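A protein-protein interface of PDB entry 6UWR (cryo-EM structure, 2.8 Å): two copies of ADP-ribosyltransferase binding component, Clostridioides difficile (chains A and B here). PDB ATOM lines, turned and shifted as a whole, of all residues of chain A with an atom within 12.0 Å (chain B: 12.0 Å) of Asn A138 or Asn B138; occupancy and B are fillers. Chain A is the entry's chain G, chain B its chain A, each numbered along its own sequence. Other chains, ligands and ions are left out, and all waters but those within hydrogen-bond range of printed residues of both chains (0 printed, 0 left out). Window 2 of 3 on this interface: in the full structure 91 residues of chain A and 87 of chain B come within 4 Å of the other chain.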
ATOM      1  N   ASN A 133     -21.546  21.647  -5.194  1.00  0.00           N
ATOM      2  CA  ASN A 133     -21.602  22.071  -6.582  1.00  0.00           C
ATOM      3  C   ASN A 133     -22.149  23.488  -6.664  1.00  0.00           C
ATOM      4  O   ASN A 133     -23.126  23.822  -5.993  1.00  0.00           O
ATOM      5  CB  ASN A 133     -22.471  21.109  -7.389  1.00  0.00           C
ATOM      6  CG  ASN A 133     -22.359  21.323  -8.873  1.00  0.00           C
ATOM      7  OD1 ASN A 133     -21.819  22.319  -9.331  1.00  0.00           O
ATOM      8  ND2 ASN A 133     -22.857  20.372  -9.638  1.00  0.00           N
ATOM      9  N   VAL A 134     -21.500  24.329  -7.464  1.00  0.00           N
ATOM     10  CA  VAL A 134     -21.995  25.660  -7.788  1.00  0.00           C
ATOM     11  C   VAL A 134     -21.822  25.865  -9.283  1.00  0.00           C
ATOM     12  O   VAL A 134     -20.837  25.419  -9.875  1.00  0.00           O
ATOM     13  CB  VAL A 134     -21.277  26.780  -7.004  1.00  0.00           C
ATOM     14  CG1 VAL A 134     -21.588  26.680  -5.538  1.00  0.00           C
ATOM     15  CG2 VAL A 134     -19.788  26.723  -7.226  1.00  0.00           C
ATOM     16  N   GLY A 135     -22.783  26.531  -9.900  1.00  0.00           N
ATOM     17  CA  GLY A 135     -22.707  26.687 -11.335  1.00  0.00           C
ATOM     18  C   GLY A 135     -23.681  27.716 -11.852  1.00  0.00           C
ATOM     19  O   GLY A 135     -24.257  28.496 -11.097  1.00  0.00           O
ATOM     20  N   TYR A 136     -23.839  27.707 -13.170  1.00  0.00           N
ATOM     21  CA  TYR A 136     -24.733  28.615 -13.871  1.00  0.00           C
ATOM     22  C   TYR A 136     -25.434  27.834 -14.967  1.00  0.00           C
ATOM     23  O   TYR A 136     -24.776  27.249 -15.827  1.00  0.00           O
ATOM     24  CB  TYR A 136     -23.965  29.798 -14.466  1.00  0.00           C
ATOM     25  CG  TYR A 136     -24.851  30.779 -15.177  1.00  0.00           C
ATOM     26  CD1 TYR A 136     -25.440  31.819 -14.496  1.00  0.00           C
ATOM     27  CD2 TYR A 136     -25.113  30.652 -16.526  1.00  0.00           C
ATOM     28  CE1 TYR A 136     -26.261  32.704 -15.133  1.00  0.00           C
ATOM     29  CE2 TYR A 136     -25.933  31.534 -17.170  1.00  0.00           C
ATOM     30  CZ  TYR A 136     -26.504  32.557 -16.467  1.00  0.00           C
ATOM     31  OH  TYR A 136     -27.323  33.448 -17.105  1.00  0.00           O
ATOM     32  N   GLN A 137     -26.762  27.817 -14.938  1.00  0.00           N
ATOM     33  CA  GLN A 137     -27.537  27.171 -15.995  1.00  0.00           C
ATOM     34  C   GLN A 137     -28.895  27.858 -16.055  1.00  0.00           C
ATOM     35  O   GLN A 137     -29.799  27.506 -15.295  1.00  0.00           O
ATOM     36  CB  GLN A 137     -27.679  25.684 -15.725  1.00  0.00           C
ATOM     37  CG  GLN A 137     -28.540  24.956 -16.718  1.00  0.00           C
ATOM     38  CD  GLN A 137     -28.585  23.479 -16.440  1.00  0.00           C
ATOM     39  OE1 GLN A 137     -28.497  23.052 -15.291  1.00  0.00           O
ATOM     40  NE2 GLN A 137     -28.712  22.684 -17.491  1.00  0.00           N
ATOM     41  N   ASN A 138     -29.038  28.812 -16.974  1.00  0.00           N
ATOM     42  CA  ASN A 138     -30.211  29.682 -17.018  1.00  0.00           C
ATOM     43  C   ASN A 138     -30.443  30.335 -15.661  1.00  0.00           C
ATOM     44  O   ASN A 138     -31.576  30.487 -15.203  1.00  0.00           O
ATOM     45  CB  ASN A 138     -31.456  28.918 -17.471  1.00  0.00           C
ATOM     46  CG  ASN A 138     -31.528  28.754 -18.972  1.00  0.00           C
ATOM     47  OD1 ASN A 138     -31.440  27.643 -19.488  1.00  0.00           O
ATOM     48  ND2 ASN A 138     -31.696  29.861 -19.682  1.00  0.00           N
ATOM     49  N   GLY A 139     -29.355  30.723 -15.010  1.00  0.00           N
ATOM     50  CA  GLY A 139     -29.389  31.217 -13.651  1.00  0.00           C
ATOM     51  C   GLY A 139     -28.370  30.511 -12.785  1.00  0.00           C
ATOM     52  O   GLY A 139     -27.773  29.508 -13.163  1.00  0.00           O
ATOM     53  N   PHE A 140     -28.187  31.061 -11.594  1.00  0.00           N
ATOM     54  CA  PHE A 140     -27.178  30.565 -10.673  1.00  0.00           C
ATOM     55  C   PHE A 140     -27.743  29.429  -9.835  1.00  0.00           C
ATOM     56  O   PHE A 140     -28.852  29.532  -9.308  1.00  0.00           O
ATOM     57  CB  PHE A 140     -26.670  31.693  -9.782  1.00  0.00           C
ATOM     58  CG  PHE A 140     -25.808  32.673 -10.500  1.00  0.00           C
ATOM     59  CD1 PHE A 140     -24.449  32.685 -10.305  1.00  0.00           C
ATOM     60  CD2 PHE A 140     -26.352  33.573 -11.386  1.00  0.00           C
ATOM     61  CE1 PHE A 140     -23.653  33.582 -10.972  1.00  0.00           C
ATOM     62  CE2 PHE A 140     -25.559  34.471 -12.053  1.00  0.00           C
ATOM     63  CZ  PHE A 140     -24.211  34.475 -11.844  1.00  0.00           C
ATOM     64  N   THR A 141     -26.979  28.349  -9.721  1.00  0.00           N
ATOM     65  CA  THR A 141     -27.399  27.135  -9.042  1.00  0.00           C
ATOM     66  C   THR A 141     -26.445  26.815  -7.896  1.00  0.00           C
ATOM     67  O   THR A 141     -25.402  27.446  -7.732  1.00  0.00           O
ATOM     68  CB  THR A 141     -27.463  25.958 -10.021  1.00  0.00           C
ATOM     69  OG1 THR A 141     -26.137  25.535 -10.349  1.00  0.00           O
ATOM     70  CG2 THR A 141     -28.175  26.356 -11.295  1.00  0.00           C
ATOM     71  N   ALA A 142     -26.826  25.825  -7.091  1.00  0.00           N
ATOM     72  CA  ALA A 142     -25.994  25.320  -6.008  1.00  0.00           C
ATOM     73  C   ALA A 142     -26.592  24.019  -5.500  1.00  0.00           C
ATOM     74  O   ALA A 142     -27.811  23.871  -5.453  1.00  0.00           O
ATOM     75  CB  ALA A 142     -25.876  26.325  -4.864  1.00  0.00           C
ATOM     76  N   ASN A 143     -25.724  23.077  -5.133  1.00  0.00           N
ATOM     77  CA  ASN A 143     -26.144  21.799  -4.571  1.00  0.00           C
ATOM     78  C   ASN A 143     -25.198  21.405  -3.454  1.00  0.00           C
ATOM     79  O   ASN A 143     -24.045  21.831  -3.421  1.00  0.00           O
ATOM     80  CB  ASN A 143     -26.140  20.662  -5.591  1.00  0.00           C
ATOM     81  CG  ASN A 143     -26.915  20.982  -6.822  1.00  0.00           C
ATOM     82  OD1 ASN A 143     -28.039  21.467  -6.757  1.00  0.00           O
ATOM     83  ND2 ASN A 143     -26.322  20.706  -7.970  1.00  0.00           N
ATOM     84  N   VAL B 134     -29.613  18.533  -1.479  1.00  0.00           N
ATOM     85  CA  VAL B 134     -30.430  19.734  -1.364  1.00  0.00           C
ATOM     86  C   VAL B 134     -29.748  20.833  -2.158  1.00  0.00           C
ATOM     87  O   VAL B 134     -28.520  20.931  -2.181  1.00  0.00           O
ATOM     88  CB  VAL B 134     -30.650  20.180   0.097  1.00  0.00           C
ATOM     89  CG1 VAL B 134     -31.474  19.167   0.840  1.00  0.00           C
ATOM     90  CG2 VAL B 134     -29.333  20.392   0.798  1.00  0.00           C
ATOM     91  N   GLY B 135     -30.541  21.659  -2.821  1.00  0.00           N
ATOM     92  CA  GLY B 135     -29.940  22.676  -3.654  1.00  0.00           C
ATOM     93  C   GLY B 135     -30.935  23.721  -4.089  1.00  0.00           C
ATOM     94  O   GLY B 135     -32.043  23.815  -3.565  1.00  0.00           O
ATOM     95  N   TYR B 136     -30.505  24.518  -5.059  1.00  0.00           N
ATOM     96  CA  TYR B 136     -31.308  25.590  -5.626  1.00  0.00           C
ATOM     97  C   TYR B 136     -31.087  25.603  -7.128  1.00  0.00           C
ATOM     98  O   TYR B 136     -29.951  25.732  -7.582  1.00  0.00           O
ATOM     99  CB  TYR B 136     -30.933  26.944  -5.019  1.00  0.00           C
ATOM    100  CG  TYR B 136     -31.757  28.079  -5.554  1.00  0.00           C
ATOM    101  CD1 TYR B 136     -32.952  28.421  -4.964  1.00  0.00           C
ATOM    102  CD2 TYR B 136     -31.348  28.795  -6.660  1.00  0.00           C
ATOM    103  CE1 TYR B 136     -33.715  29.441  -5.457  1.00  0.00           C
ATOM    104  CE2 TYR B 136     -32.105  29.816  -7.157  1.00  0.00           C
ATOM    105  CZ  TYR B 136     -33.288  30.134  -6.552  1.00  0.00           C
ATOM    106  OH  TYR B 136     -34.050  31.159  -7.039  1.00  0.00           O
ATOM    107  N   GLN B 137     -32.163  25.465  -7.896  1.00  0.00           N
ATOM    108  CA  GLN B 137     -32.072  25.553  -9.351  1.00  0.00           C
ATOM    109  C   GLN B 137     -33.427  26.018  -9.868  1.00  0.00           C
ATOM    110  O   GLN B 137     -34.328  25.198 -10.058  1.00  0.00           O
ATOM    111  CB  GLN B 137     -31.680  24.213  -9.947  1.00  0.00           C
ATOM    112  CG  GLN B 137     -31.653  24.191 -11.449  1.00  0.00           C
ATOM    113  CD  GLN B 137     -31.190  22.862 -11.980  1.00  0.00           C
ATOM    114  OE1 GLN B 137     -31.425  21.824 -11.366  1.00  0.00           O
ATOM    115  NE2 GLN B 137     -30.518  22.882 -13.121  1.00  0.00           N
ATOM    116  N   ASN B 138     -33.553  27.320 -10.117  1.00  0.00           N
ATOM    117  CA  ASN B 138     -34.843  27.932 -10.429  1.00  0.00           C
ATOM    118  C   ASN B 138     -35.873  27.583  -9.363  1.00  0.00           C
ATOM    119  O   ASN B 138     -37.041  27.326  -9.653  1.00  0.00           O
ATOM    120  CB  ASN B 138     -35.337  27.516 -11.816  1.00  0.00           C
ATOM    121  CG  ASN B 138     -34.696  28.313 -12.929  1.00  0.00           C
ATOM    122  OD1 ASN B 138     -33.944  27.773 -13.737  1.00  0.00           O
ATOM    123  ND2 ASN B 138     -34.992  29.604 -12.983  1.00  0.00           N
ATOM    124  N   GLY B 139     -35.432  27.570  -8.113  1.00  0.00           N
ATOM    125  CA  GLY B 139     -36.238  27.111  -7.002  1.00  0.00           C
ATOM    126  C   GLY B 139     -35.486  26.104  -6.159  1.00  0.00           C
ATOM    127  O   GLY B 139     -34.428  25.604  -6.525  1.00  0.00           O
ATOM    128  N   PHE B 140     -36.070  25.811  -5.005  1.00  0.00           N
ATOM    129  CA  PHE B 140     -35.437  24.933  -4.035  1.00  0.00           C
ATOM    130  C   PHE B 140     -35.772  23.482  -4.340  1.00  0.00           C
ATOM    131  O   PHE B 140     -36.929  23.146  -4.594  1.00  0.00           O
ATOM    132  CB  PHE B 140     -35.875  25.303  -2.622  1.00  0.00           C
ATOM    133  CG  PHE B 140     -35.285  26.582  -2.134  1.00  0.00           C
ATOM    134  CD1 PHE B 140     -34.277  26.580  -1.202  1.00  0.00           C
ATOM    135  CD2 PHE B 140     -35.727  27.791  -2.623  1.00  0.00           C
ATOM    136  CE1 PHE B 140     -33.730  27.758  -0.761  1.00  0.00           C
ATOM    137  CE2 PHE B 140     -35.182  28.968  -2.181  1.00  0.00           C
ATOM    138  CZ  PHE B 140     -34.185  28.950  -1.250  1.00  0.00           C
ATOM    139  N   THR B 141     -34.754  22.630  -4.319  1.00  0.00           N
ATOM    140  CA  THR B 141     -34.872  21.227  -4.680  1.00  0.00           C
ATOM    141  C   THR B 141     -34.452  20.344  -3.510  1.00  0.00           C
ATOM    142  O   THR B 141     -33.944  20.819  -2.495  1.00  0.00           O
ATOM    143  CB  THR B 141     -34.020  20.910  -5.915  1.00  0.00           C
ATOM    144  OG1 THR B 141     -32.638  20.890  -5.550  1.00  0.00           O
ATOM    145  CG2 THR B 141     -34.225  21.954  -6.991  1.00  0.00           C
ATOM    146  N   ALA B 142     -34.685  19.042  -3.661  1.00  0.00           N
ATOM    147  CA  ALA B 142     -34.260  18.044  -2.690  1.00  0.00           C
ATOM    148  C   ALA B 142     -34.413  16.665  -3.311  1.00  0.00           C
ATOM    149  O   ALA B 142     -35.353  16.421  -4.063  1.00  0.00           O
ATOM    150  CB  ALA B 142     -35.065  18.129  -1.394  1.00  0.00           C
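Along chain A the printed residues that touch a printed residue of chain B span positions 137 to 143. Among the printed residues, 8 pairs touch across the chains. Among the printed residues, no Asp or Glu carboxylate lies within 4 Å of a Lys or Arg side-chain nitrogen of the other chain.
Asn B138 touches its own counterpart, Asn A138. Phe A140 touches Tyr B136, but with the chains exchanged Tyr A136 does not touch Phe B140 (14.7 Å). Thr A141 touches Tyr B136, but with the chains exchanged Tyr A136 does not touch Thr B141 (13.2 Å). Ala A142 touches Tyr B136, but with the chains exchanged Tyr A136 does not touch Ala B142 (16.8 Å).
Asn B138 touches Asn A138. Phe A140 touches Tyr B136 (O to CD2, 3.7 Å). O of Tyr B136 touches CA of Thr A141, at 3.3 Å. Ala A142 touches Gly B135 (O to CA, 3.0 Å). Asn A143 touches Val B134 (CA to O, 3.5 Å). Gly B135 touches Asn A143.
N of Tyr B136 is in hydrogen-bond range of O of Ala A142, at 2.8 Å. The side-chain amide nitrogen (NE2) of Gln B137 lies within hydrogen-bond range of the side-chain amide oxygen (OE1) of Gln A137.
Of chain B, only Asn B138 (3.9 Å) comes within 4 Å of Asn A138. Asn B138 touches just one residue of chain A: Asn A138 (3.9 Å). Of chain B, only Gln B137 (3.0 Å) comes within 4 Å of Gln A137. Gly A139 touches none of the printed residues of chain B. Tyr B136 touches just these residues of chain A: Phe A140, Thr A141 and Ala A142. Gln B137 touches just one residue of chain A: Gln A137. Gly B139 touches none of the printed residues of chain A. Of the printed residues of chain A, Gly B135 touches Ala A142 (3.0 Å) and Asn A143 (3.8 Å). Of the printed residues of chain B, Thr A141 touches Tyr B136 (3.3 Å). Printed residues of chain B within 4 Å of Asn A143: Val B134 and Gly B135. Thr B141 touches none of the printed residues of chain A. The nearest residue of chain A that does not touch Asn B138 is Gln A137 (4.4 Å). The nearest printed residue of chain A that does not touch Val B134 is Ala A142 (4.5 Å).
The backbone NH (N) of Thr B141 sits at hydrogen-bond distance from the backbone carbonyl oxygen (O) of Gly B135 (3.1 Å). The backbone NH (N) of Asn A143 sits at hydrogen-bond distance from the backbone carbonyl oxygen (O) of Asn A133. The backbone carbonyl oxygen (O) of Gly A135 lies within hydrogen-bond range of the backbone NH (N) of Thr A141.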
